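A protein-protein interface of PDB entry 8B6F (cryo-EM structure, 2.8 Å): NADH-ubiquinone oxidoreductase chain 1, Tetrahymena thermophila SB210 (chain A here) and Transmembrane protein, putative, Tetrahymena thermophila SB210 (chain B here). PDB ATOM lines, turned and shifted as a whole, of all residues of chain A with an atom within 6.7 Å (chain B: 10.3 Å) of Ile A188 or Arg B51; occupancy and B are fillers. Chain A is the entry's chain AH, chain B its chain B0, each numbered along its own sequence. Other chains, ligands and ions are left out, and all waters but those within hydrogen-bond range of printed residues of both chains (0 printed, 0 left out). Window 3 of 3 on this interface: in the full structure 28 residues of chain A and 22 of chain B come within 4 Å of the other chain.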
ATOM      1  N   PRO A 112      17.540  -8.507  23.844  1.00  0.00           N
ATOM      2  CA  PRO A 112      17.805  -9.465  22.758  1.00  0.00           C
ATOM      3  C   PRO A 112      18.969 -10.396  23.052  1.00  0.00           C
ATOM      4  O   PRO A 112      18.889 -11.592  22.751  1.00  0.00           O
ATOM      5  CB  PRO A 112      18.086  -8.554  21.555  1.00  0.00           C
ATOM      6  CG  PRO A 112      17.389  -7.280  21.873  1.00  0.00           C
ATOM      7  CD  PRO A 112      17.483  -7.120  23.358  1.00  0.00           C
ATOM      8  N   SER A 113      20.056  -9.879  23.630  1.00  0.00           N
ATOM      9  CA  SER A 113      21.179 -10.712  24.039  1.00  0.00           C
ATOM     10  C   SER A 113      21.756 -10.249  25.370  1.00  0.00           C
ATOM     11  O   SER A 113      22.940 -10.467  25.649  1.00  0.00           O
ATOM     12  CB  SER A 113      22.264 -10.730  22.967  1.00  0.00           C
ATOM     13  OG  SER A 113      21.756 -11.318  21.784  1.00  0.00           O
ATOM     14  N   SER A 178       8.795 -21.245  18.512  1.00  0.00           N
ATOM     15  CA  SER A 178      10.107 -20.609  18.590  1.00  0.00           C
ATOM     16  C   SER A 178      11.177 -21.451  17.907  1.00  0.00           C
ATOM     17  O   SER A 178      12.042 -20.913  17.205  1.00  0.00           O
ATOM     18  CB  SER A 178      10.481 -20.362  20.048  1.00  0.00           C
ATOM     19  OG  SER A 178      10.584 -21.589  20.747  1.00  0.00           O
ATOM     20  N   SER A 180      13.501 -23.078  19.519  1.00  0.00           N
ATOM     21  CA  SER A 180      14.737 -22.975  20.281  1.00  0.00           C
ATOM     22  C   SER A 180      14.402 -22.892  21.760  1.00  0.00           C
ATOM     23  O   SER A 180      13.276 -22.568  22.144  1.00  0.00           O
ATOM     24  CB  SER A 180      15.548 -21.748  19.883  1.00  0.00           C
ATOM     25  OG  SER A 180      14.825 -20.591  20.242  1.00  0.00           O
ATOM     26  N   CYS A 182      16.184 -20.818  23.691  1.00  0.00           N
ATOM     27  CA  CYS A 182      16.583 -19.485  24.115  1.00  0.00           C
ATOM     28  C   CYS A 182      15.370 -18.573  24.235  1.00  0.00           C
ATOM     29  O   CYS A 182      14.450 -18.624  23.415  1.00  0.00           O
ATOM     30  CB  CYS A 182      17.584 -18.889  23.125  1.00  0.00           C
ATOM     31  SG  CYS A 182      18.254 -17.287  23.619  1.00  0.00           S
ATOM     32  N   PHE A 183      15.376 -17.732  25.269  1.00  0.00           N
ATOM     33  CA  PHE A 183      14.257 -16.825  25.494  1.00  0.00           C
ATOM     34  C   PHE A 183      14.144 -15.764  24.405  1.00  0.00           C
ATOM     35  O   PHE A 183      13.041 -15.283  24.127  1.00  0.00           O
ATOM     36  CB  PHE A 183      14.396 -16.151  26.860  1.00  0.00           C
ATOM     37  CG  PHE A 183      14.314 -17.097  28.023  1.00  0.00           C
ATOM     38  CD1 PHE A 183      13.492 -18.211  27.980  1.00  0.00           C
ATOM     39  CD2 PHE A 183      15.050 -16.857  29.170  1.00  0.00           C
ATOM     40  CE1 PHE A 183      13.415 -19.073  29.054  1.00  0.00           C
ATOM     41  CE2 PHE A 183      14.976 -17.715  30.248  1.00  0.00           C
ATOM     42  CZ  PHE A 183      14.156 -18.824  30.191  1.00  0.00           C
ATOM     43  N   SER A 184      15.262 -15.382  23.787  1.00  0.00           N
ATOM     44  CA  SER A 184      15.229 -14.292  22.816  1.00  0.00           C
ATOM     45  C   SER A 184      14.359 -14.636  21.615  1.00  0.00           C
ATOM     46  O   SER A 184      13.629 -13.782  21.101  1.00  0.00           O
ATOM     47  CB  SER A 184      16.646 -13.959  22.359  1.00  0.00           C
ATOM     48  OG  SER A 184      17.458 -13.579  23.451  1.00  0.00           O
ATOM     49  N   VAL A 185      14.425 -15.884  21.151  1.00  0.00           N
ATOM     50  CA  VAL A 185      13.751 -16.267  19.916  1.00  0.00           C
ATOM     51  C   VAL A 185      12.239 -16.132  20.022  1.00  0.00           C
ATOM     52  O   VAL A 185      11.552 -16.094  18.997  1.00  0.00           O
ATOM     53  CB  VAL A 185      14.188 -17.687  19.508  1.00  0.00           C
ATOM     54  CG1 VAL A 185      13.545 -18.102  18.196  1.00  0.00           C
ATOM     55  CG2 VAL A 185      15.707 -17.710  19.368  1.00  0.00           C
ATOM     56  N   PHE A 186      11.696 -16.063  21.236  1.00  0.00           N
ATOM     57  CA  PHE A 186      10.252 -15.919  21.377  1.00  0.00           C
ATOM     58  C   PHE A 186       9.803 -14.501  21.048  1.00  0.00           C
ATOM     59  O   PHE A 186       8.756 -14.309  20.423  1.00  0.00           O
ATOM     60  CB  PHE A 186       9.818 -16.296  22.793  1.00  0.00           C
ATOM     61  CG  PHE A 186      10.044 -17.737  23.130  1.00  0.00           C
ATOM     62  CD1 PHE A 186      11.268 -18.170  23.608  1.00  0.00           C
ATOM     63  CD2 PHE A 186       9.024 -18.661  22.980  1.00  0.00           C
ATOM     64  CE1 PHE A 186      11.474 -19.500  23.922  1.00  0.00           C
ATOM     65  CE2 PHE A 186       9.221 -19.989  23.292  1.00  0.00           C
ATOM     66  CZ  PHE A 186      10.448 -20.409  23.764  1.00  0.00           C
ATOM     67  N   VAL A 187      10.583 -13.500  21.454  1.00  0.00           N
ATOM     68  CA  VAL A 187      10.151 -12.113  21.318  1.00  0.00           C
ATOM     69  C   VAL A 187      10.055 -11.714  19.850  1.00  0.00           C
ATOM     70  O   VAL A 187       9.171 -10.943  19.462  1.00  0.00           O
ATOM     71  CB  VAL A 187      11.093 -11.182  22.101  1.00  0.00           C
ATOM     72  CG1 VAL A 187      10.708  -9.728  21.881  1.00  0.00           C
ATOM     73  CG2 VAL A 187      11.047 -11.526  23.578  1.00  0.00           C
ATOM     74  N   ILE A 188      10.961 -12.220  19.011  1.00  0.00           N
ATOM     75  CA  ILE A 188      10.938 -11.856  17.595  1.00  0.00           C
ATOM     76  C   ILE A 188       9.622 -12.280  16.958  1.00  0.00           C
ATOM     77  O   ILE A 188       9.079 -11.575  16.099  1.00  0.00           O
ATOM     78  CB  ILE A 188      12.149 -12.460  16.858  1.00  0.00           C
ATOM     79  CG1 ILE A 188      12.187 -13.981  17.021  1.00  0.00           C
ATOM     80  CG2 ILE A 188      13.434 -11.834  17.375  1.00  0.00           C
ATOM     81  CD1 ILE A 188      13.234 -14.667  16.169  1.00  0.00           C
ATOM     82  N   TYR A 189       9.092 -13.436  17.357  1.00  0.00           N
ATOM     83  CA  TYR A 189       7.788 -13.867  16.867  1.00  0.00           C
ATOM     84  C   TYR A 189       6.645 -13.125  17.546  1.00  0.00           C
ATOM     85  O   TYR A 189       5.599 -12.911  16.927  1.00  0.00           O
ATOM     86  CB  TYR A 189       7.619 -15.372  17.074  1.00  0.00           C
ATOM     87  CG  TYR A 189       8.557 -16.207  16.236  1.00  0.00           C
ATOM     88  CD1 TYR A 189       8.354 -16.355  14.872  1.00  0.00           C
ATOM     89  CD2 TYR A 189       9.642 -16.852  16.811  1.00  0.00           C
ATOM     90  CE1 TYR A 189       9.207 -17.117  14.102  1.00  0.00           C
ATOM     91  CE2 TYR A 189      10.503 -17.617  16.051  1.00  0.00           C
ATOM     92  CZ  TYR A 189      10.280 -17.746  14.697  1.00  0.00           C
ATOM     93  OH  TYR A 189      11.133 -18.509  13.933  1.00  0.00           O
ATOM     94  N   GLN A 190       6.821 -12.729  18.804  1.00  0.00           N
ATOM     95  CA  GLN A 190       5.772 -12.058  19.560  1.00  0.00           C
ATOM     96  C   GLN A 190       5.695 -10.561  19.290  1.00  0.00           C
ATOM     97  O   GLN A 190       4.850  -9.888  19.887  1.00  0.00           O
ATOM     98  CB  GLN A 190       5.981 -12.290  21.057  1.00  0.00           C
ATOM     99  CG  GLN A 190       5.782 -13.728  21.484  1.00  0.00           C
ATOM    100  CD  GLN A 190       6.069 -13.936  22.954  1.00  0.00           C
ATOM    101  OE1 GLN A 190       5.219 -14.413  23.700  1.00  0.00           O
ATOM    102  NE2 GLN A 190       7.276 -13.580  23.378  1.00  0.00           N
ATOM    103  N   GLU A 191       6.554 -10.019  18.424  1.00  0.00           N
ATOM    104  CA  GLU A 191       6.514  -8.588  18.141  1.00  0.00           C
ATOM    105  C   GLU A 191       5.127  -8.152  17.680  1.00  0.00           C
ATOM    106  O   GLU A 191       4.578  -7.165  18.181  1.00  0.00           O
ATOM    107  CB  GLU A 191       7.565  -8.229  17.089  1.00  0.00           C
ATOM    108  CG  GLU A 191       9.002  -8.396  17.567  1.00  0.00           C
ATOM    109  CD  GLU A 191      10.012  -7.812  16.596  1.00  0.00           C
ATOM    110  OE1 GLU A 191       9.592  -7.283  15.547  1.00  0.00           O
ATOM    111  OE2 GLU A 191      11.226  -7.882  16.884  1.00  0.00           O
ATOM    112  N   ILE A 192       4.543  -8.875  16.725  1.00  0.00           N
ATOM    113  CA  ILE A 192       3.258  -8.461  16.162  1.00  0.00           C
ATOM    114  C   ILE A 192       2.118  -8.809  17.114  1.00  0.00           C
ATOM    115  O   ILE A 192       1.325  -7.944  17.499  1.00  0.00           O
ATOM    116  CB  ILE A 192       3.050  -9.089  14.772  1.00  0.00           C
ATOM    117  CG1 ILE A 192       4.141  -8.604  13.814  1.00  0.00           C
ATOM    118  CG2 ILE A 192       1.672  -8.736  14.224  1.00  0.00           C
ATOM    119  CD1 ILE A 192       4.092  -9.236  12.438  1.00  0.00           C
ATOM    120  N   GLY A 265       5.107 -11.492  25.081  1.00  0.00           N
ATOM    121  CA  GLY A 265       5.917 -10.568  24.319  1.00  0.00           C
ATOM    122  C   GLY A 265       7.215 -10.156  24.970  1.00  0.00           C
ATOM    123  O   GLY A 265       8.021  -9.475  24.324  1.00  0.00           O
ATOM    124  N   TRP A 267       9.781  -8.123  26.181  1.00  0.00           N
ATOM    125  CA  TRP A 267      10.098  -6.701  26.183  1.00  0.00           C
ATOM    126  C   TRP A 267       9.483  -5.968  24.995  1.00  0.00           C
ATOM    127  O   TRP A 267      10.012  -4.940  24.560  1.00  0.00           O
ATOM    128  CB  TRP A 267      11.612  -6.500  26.211  1.00  0.00           C
ATOM    129  CG  TRP A 267      12.359  -7.327  25.207  1.00  0.00           C
ATOM    130  CD1 TRP A 267      12.583  -7.020  23.898  1.00  0.00           C
ATOM    131  CD2 TRP A 267      12.981  -8.596  25.433  1.00  0.00           C
ATOM    132  NE1 TRP A 267      13.306  -8.020  23.295  1.00  0.00           N
ATOM    133  CE2 TRP A 267      13.561  -9.000  24.216  1.00  0.00           C
ATOM    134  CE3 TRP A 267      13.102  -9.432  26.549  1.00  0.00           C
ATOM    135  CZ2 TRP A 267      14.254 -10.202  24.081  1.00  0.00           C
ATOM    136  CZ3 TRP A 267      13.788 -10.625  26.414  1.00  0.00           C
ATOM    137  CH2 TRP A 267      14.355 -10.999  25.188  1.00  0.00           C
ATOM    138  N   GLU A 268       8.376  -6.477  24.463  1.00  0.00           N
ATOM    139  CA  GLU A 268       7.648  -5.834  23.379  1.00  0.00           C
ATOM    140  C   GLU A 268       6.348  -5.255  23.918  1.00  0.00           C
ATOM    141  O   GLU A 268       5.602  -5.945  24.619  1.00  0.00           O
ATOM    142  CB  GLU A 268       7.360  -6.825  22.250  1.00  0.00           C
ATOM    143  CG  GLU A 268       8.565  -7.137  21.378  1.00  0.00           C
ATOM    144  CD  GLU A 268       9.012  -5.947  20.547  1.00  0.00           C
ATOM    145  OE1 GLU A 268       8.292  -4.928  20.528  1.00  0.00           O
ATOM    146  OE2 GLU A 268      10.085  -6.030  19.916  1.00  0.00           O
ATOM    147  N   ILE B  45      26.669  -4.906  22.803  1.00  0.00           N
ATOM    148  CA  ILE B  45      25.900  -6.091  23.177  1.00  0.00           C
ATOM    149  C   ILE B  45      25.973  -7.026  21.975  1.00  0.00           C
ATOM    150  O   ILE B  45      25.137  -6.983  21.072  1.00  0.00           O
ATOM    151  CB  ILE B  45      24.463  -5.749  23.560  1.00  0.00           C
ATOM    152  CG1 ILE B  45      24.432  -4.753  24.722  1.00  0.00           C
ATOM    153  CG2 ILE B  45      23.694  -7.017  23.916  1.00  0.00           C
ATOM    154  CD1 ILE B  45      25.042  -5.268  26.010  1.00  0.00           C
ATOM    155  N   GLU B  46      26.991  -7.882  21.960  1.00  0.00           N
ATOM    156  CA  GLU B  46      27.168  -8.799  20.844  1.00  0.00           C
ATOM    157  C   GLU B  46      26.048  -9.828  20.824  1.00  0.00           C
ATOM    158  O   GLU B  46      25.673 -10.386  21.858  1.00  0.00           O
ATOM    159  CB  GLU B  46      28.522  -9.503  20.933  1.00  0.00           C
ATOM    160  CG  GLU B  46      28.695 -10.385  22.159  1.00  0.00           C
ATOM    161  CD  GLU B  46      29.950 -11.229  22.088  1.00  0.00           C
ATOM    162  OE1 GLU B  46      30.685 -11.117  21.084  1.00  0.00           O
ATOM    163  OE2 GLU B  46      30.203 -12.006  23.032  1.00  0.00           O
ATOM    164  N   ARG B  47      25.514 -10.080  19.632  1.00  0.00           N
ATOM    165  CA  ARG B  47      24.493 -11.106  19.490  1.00  0.00           C
ATOM    166  C   ARG B  47      25.069 -12.472  19.837  1.00  0.00           C
ATOM    167  O   ARG B  47      26.249 -12.751  19.611  1.00  0.00           O
ATOM    168  CB  ARG B  47      23.936 -11.113  18.065  1.00  0.00           C
ATOM    169  CG  ARG B  47      23.387  -9.767  17.621  1.00  0.00           C
ATOM    170  CD  ARG B  47      22.567  -9.875  16.344  1.00  0.00           C
ATOM    171  NE  ARG B  47      23.362 -10.308  15.201  1.00  0.00           N
ATOM    172  CZ  ARG B  47      23.488 -11.566  14.798  1.00  0.00           C
ATOM    173  NH1 ARG B  47      22.890 -12.561  15.434  1.00  0.00           N
ATOM    174  NH2 ARG B  47      24.234 -11.834  13.732  1.00  0.00           N
ATOM    175  N   PHE B  48      24.222 -13.330  20.400  1.00  0.00           N
ATOM    176  CA  PHE B  48      24.662 -14.673  20.745  1.00  0.00           C
ATOM    177  C   PHE B  48      25.161 -15.394  19.502  1.00  0.00           C
ATOM    178  O   PHE B  48      24.663 -15.194  18.392  1.00  0.00           O
ATOM    179  CB  PHE B  48      23.525 -15.472  21.385  1.00  0.00           C
ATOM    180  CG  PHE B  48      23.158 -15.025  22.777  1.00  0.00           C
ATOM    181  CD1 PHE B  48      24.052 -14.318  23.564  1.00  0.00           C
ATOM    182  CD2 PHE B  48      21.913 -15.330  23.298  1.00  0.00           C
ATOM    183  CE1 PHE B  48      23.709 -13.922  24.839  1.00  0.00           C
ATOM    184  CE2 PHE B  48      21.565 -14.936  24.572  1.00  0.00           C
ATOM    185  CZ  PHE B  48      22.463 -14.231  25.343  1.00  0.00           C
ATOM    186  N   TYR B  49      26.168 -16.243  19.703  1.00  0.00           N
ATOM    187  CA  TYR B  49      26.764 -16.956  18.580  1.00  0.00           C
ATOM    188  C   TYR B  49      25.741 -17.838  17.879  1.00  0.00           C
ATOM    189  O   TYR B  49      25.683 -17.871  16.645  1.00  0.00           O
ATOM    190  CB  TYR B  49      27.945 -17.787  19.074  1.00  0.00           C
ATOM    191  CG  TYR B  49      28.613 -18.593  17.995  1.00  0.00           C
ATOM    192  CD1 TYR B  49      29.484 -17.995  17.100  1.00  0.00           C
ATOM    193  CD2 TYR B  49      28.386 -19.955  17.881  1.00  0.00           C
ATOM    194  CE1 TYR B  49      30.102 -18.724  16.117  1.00  0.00           C
ATOM    195  CE2 TYR B  49      29.001 -20.695  16.901  1.00  0.00           C
ATOM    196  CZ  TYR B  49      29.858 -20.073  16.024  1.00  0.00           C
ATOM    197  OH  TYR B  49      30.468 -20.810  15.045  1.00  0.00           O
ATOM    198  N   PHE B  50      24.918 -18.553  18.647  1.00  0.00           N
ATOM    199  CA  PHE B  50      23.934 -19.452  18.059  1.00  0.00           C
ATOM    200  C   PHE B  50      22.768 -18.717  17.414  1.00  0.00           C
ATOM    201  O   PHE B  50      22.006 -19.340  16.668  1.00  0.00           O
ATOM    202  CB  PHE B  50      23.409 -20.422  19.120  1.00  0.00           C
ATOM    203  CG  PHE B  50      22.822 -19.748  20.323  1.00  0.00           C
ATOM    204  CD1 PHE B  50      21.485 -19.392  20.351  1.00  0.00           C
ATOM    205  CD2 PHE B  50      23.607 -19.480  21.433  1.00  0.00           C
ATOM    206  CE1 PHE B  50      20.942 -18.775  21.459  1.00  0.00           C
ATOM    207  CE2 PHE B  50      23.072 -18.865  22.544  1.00  0.00           C
ATOM    208  CZ  PHE B  50      21.738 -18.512  22.557  1.00  0.00           C
ATOM    209  N   ARG B  51      22.607 -17.424  17.677  1.00  0.00           N
ATOM    210  CA  ARG B  51      21.592 -16.614  17.008  1.00  0.00           C
ATOM    211  C   ARG B  51      22.142 -16.014  15.720  1.00  0.00           C
ATOM    212  O   ARG B  51      22.070 -14.808  15.495  1.00  0.00           O
ATOM    213  CB  ARG B  51      21.095 -15.518  17.941  1.00  0.00           C
ATOM    214  CG  ARG B  51      20.443 -16.017  19.215  1.00  0.00           C
ATOM    215  CD  ARG B  51      19.139 -16.752  18.949  1.00  0.00           C
ATOM    216  NE  ARG B  51      18.198 -15.954  18.169  1.00  0.00           N
ATOM    217  CZ  ARG B  51      17.817 -16.221  16.925  1.00  0.00           C
ATOM    218  NH1 ARG B  51      18.261 -17.283  16.271  1.00  0.00           N
ATOM    219  NH2 ARG B  51      16.956 -15.406  16.324  1.00  0.00           N
ATOM    220  N   SER B  52      22.704 -16.858  14.860  1.00  0.00           N
ATOM    221  CA  SER B  52      23.361 -16.370  13.657  1.00  0.00           C
ATOM    222  C   SER B  52      23.414 -17.495  12.635  1.00  0.00           C
ATOM    223  O   SER B  52      23.382 -18.677  12.982  1.00  0.00           O
ATOM    224  CB  SER B  52      24.769 -15.854  13.975  1.00  0.00           C
ATOM    225  OG  SER B  52      25.299 -15.104  12.899  1.00  0.00           O
ATOM    226  N   SER B  53      23.499 -17.106  11.365  1.00  0.00           N
ATOM    227  CA  SER B  53      23.584 -18.075  10.286  1.00  0.00           C
ATOM    228  C   SER B  53      24.951 -18.757  10.286  1.00  0.00           C
ATOM    229  O   SER B  53      25.901 -18.311  10.932  1.00  0.00           O
ATOM    230  CB  SER B  53      23.343 -17.398   8.938  1.00  0.00           C
ATOM    231  OG  SER B  53      22.148 -16.644   8.953  1.00  0.00           O
ATOM    232  N   LYS B  54      25.045 -19.853   9.531  1.00  0.00           N
ATOM    233  CA  LYS B  54      26.310 -20.573   9.438  1.00  0.00           C
ATOM    234  C   LYS B  54      27.393 -19.683   8.844  1.00  0.00           C
ATOM    235  O   LYS B  54      28.512 -19.614   9.362  1.00  0.00           O
ATOM    236  CB  LYS B  54      26.127 -21.840   8.602  1.00  0.00           C
ATOM    237  CG  LYS B  54      27.366 -22.717   8.503  1.00  0.00           C
ATOM    238  CD  LYS B  54      27.731 -23.333   9.842  1.00  0.00           C
ATOM    239  CE  LYS B  54      28.911 -24.285   9.710  1.00  0.00           C
ATOM    240  NZ  LYS B  54      28.616 -25.428   8.802  1.00  0.00           N
ATOM    241  N   PHE B  55      27.074 -18.985   7.753  1.00  0.00           N
ATOM    242  CA  PHE B  55      28.054 -18.101   7.133  1.00  0.00           C
ATOM    243  C   PHE B  55      28.450 -16.972   8.075  1.00  0.00           C
ATOM    244  O   PHE B  55      29.627 -16.607   8.161  1.00  0.00           O
ATOM    245  CB  PHE B  55      27.499 -17.541   5.825  1.00  0.00           C
ATOM    246  CG  PHE B  55      28.490 -16.727   5.048  1.00  0.00           C
ATOM    247  CD1 PHE B  55      28.645 -15.375   5.301  1.00  0.00           C
ATOM    248  CD2 PHE B  55      29.266 -17.313   4.065  1.00  0.00           C
ATOM    249  CE1 PHE B  55      29.556 -14.624   4.588  1.00  0.00           C
ATOM    250  CE2 PHE B  55      30.179 -16.567   3.349  1.00  0.00           C
ATOM    251  CZ  PHE B  55      30.325 -15.221   3.611  1.00  0.00           C
ATOM    252  N   GLU B  56      27.477 -16.405   8.792  1.00  0.00           N
ATOM    253  CA  GLU B  56      27.787 -15.340   9.740  1.00  0.00           C
ATOM    254  C   GLU B  56      28.693 -15.846  10.854  1.00  0.00           C
ATOM    255  O   GLU B  56      29.637 -15.156  11.256  1.00  0.00           O
ATOM    256  CB  GLU B  56      26.499 -14.758  10.320  1.00  0.00           C
ATOM    257  CG  GLU B  56      25.675 -13.966   9.319  1.00  0.00           C
ATOM    258  CD  GLU B  56      24.456 -13.322   9.949  1.00  0.00           C
ATOM    259  OE1 GLU B  56      24.433 -13.181  11.189  1.00  0.00           O
ATOM    260  OE2 GLU B  56      23.521 -12.961   9.206  1.00  0.00           O
ATOM    261  N   ARG B  57      28.427 -17.050  11.359  1.00  0.00           N
ATOM    262  CA  ARG B  57      29.287 -17.624  12.387  1.00  0.00           C
ATOM    263  C   ARG B  57      30.708 -17.794  11.871  1.00  0.00           C
ATOM    264  O   ARG B  57      31.677 -17.454  12.561  1.00  0.00           O
ATOM    265  CB  ARG B  57      28.727 -18.971  12.839  1.00  0.00           C
ATOM    266  CG  ARG B  57      27.390 -18.892  13.553  1.00  0.00           C
ATOM    267  CD  ARG B  57      26.711 -20.249  13.563  1.00  0.00           C
ATOM    268  NE  ARG B  57      25.388 -20.200  14.169  1.00  0.00           N
ATOM    269  CZ  ARG B  57      24.545 -21.223  14.207  1.00  0.00           C
ATOM    270  NH1 ARG B  57      24.854 -22.392  13.671  1.00  0.00           N
ATOM    271  NH2 ARG B  57      23.363 -21.070  14.796  1.00  0.00           N
ATOM    272  N   ARG B  60      32.402 -14.409  11.621  1.00  0.00           N
ATOM    273  CA  ARG B  60      32.718 -13.860  12.936  1.00  0.00           C
ATOM    274  C   ARG B  60      33.943 -14.529  13.545  1.00  0.00           C
ATOM    275  O   ARG B  60      34.800 -13.852  14.124  1.00  0.00           O
ATOM    276  CB  ARG B  60      31.512 -14.016  13.863  1.00  0.00           C
ATOM    277  CG  ARG B  60      30.322 -13.153  13.478  1.00  0.00           C
ATOM    278  CD  ARG B  60      29.050 -13.597  14.184  1.00  0.00           C
ATOM    279  NE  ARG B  60      29.069 -13.290  15.610  1.00  0.00           N
ATOM    280  CZ  ARG B  60      28.080 -13.566  16.448  1.00  0.00           C
ATOM    281  NH1 ARG B  60      26.975 -14.169  16.041  1.00  0.00           N
ATOM    282  NH2 ARG B  60      28.204 -13.233  17.730  1.00  0.00           N
ATOM    283  N   LYS B  61      34.049 -15.852  13.429  1.00  0.00           N
ATOM    284  CA  LYS B  61      35.110 -16.596  14.092  1.00  0.00           C
ATOM    285  C   LYS B  61      36.360 -16.769  13.240  1.00  0.00           C
ATOM    286  O   LYS B  61      37.356 -17.299  13.740  1.00  0.00           O
ATOM    287  CB  LYS B  61      34.595 -17.975  14.515  1.00  0.00           C
ATOM    288  CG  LYS B  61      33.416 -17.925  15.474  1.00  0.00           C
ATOM    289  CD  LYS B  61      33.797 -17.273  16.797  1.00  0.00           C
ATOM    290  CE  LYS B  61      32.588 -17.125  17.703  1.00  0.00           C
ATOM    291  NZ  LYS B  61      32.949 -16.512  19.010  1.00  0.00           N
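OG of Ser A113 lies within hydrogen-bond range of N of Phe B48, at 3.5 Å.
The side-chain sulfur of Cys A182 lies close to the backbone NH of Ser A184.
O of Phe B48 is in hydrogen-bond range of NH1 of Arg B60, at 3.5 Å.
O of Phe B50 sits at hydrogen-bond distance from NH2 of Arg B57 (2.9 Å).
The side-chain carboxylate of Glu B56 is in salt-bridge range of the guanidinium group of Arg B47 (2.9 Å).
The guanidinium group of Arg B60 sits at hydrogen-bond distance from the backbone carbonyl oxygen of Arg B47 (2.8 Å).
Among the printed residues, merely in contact across the chains: Val A185 with Arg B51 (3.3 Å), Ser A113 with Arg B47 (3.6 Å), Ser A113 with Glu B46 (3.6 Å), Cys A182 with Phe B50 (3.8 Å), Ile A188 with Arg B51 (3.8 Å) and Ser A113 with Ile B45 (3.9 Å).
Of the printed residues of chain B, Ser A113 touches Ile B45 (3.9 Å), Glu B46 (3.6 Å), Arg B47 (3.6 Å) and Phe B48 (3.5 Å).
Printed residues of chain B within 4 Å of Cys A182: Phe B50 (3.8 Å).
Val A185 touches just one residue of chain B: Arg B51.
No residue of chain B comes within 4 Å of Val A187.
Of chain B, only Arg B51 comes within 4 Å of Ile A188.
No residue of chain B comes within 4 Å of Tyr A189.
Of the printed residues of chain A, Glu B46 touches Ser A113 (3.6 Å).
Printed residues of chain A within 4 Å of Phe B50: Cys A182.
Arg B51 touches just these residues of chain A: Val A185 (3.3 Å) and Ile A188 (3.8 Å).
The nearest residue of chain B that does not touch Ile A188 is Arg B47 (9.4 Å).
The nearest residue of chain A that does not touch Arg B51 is Cys A182 (4.8 Å).
Of the 15 printed residues of chain B, 6 touch a printed residue of chain A.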
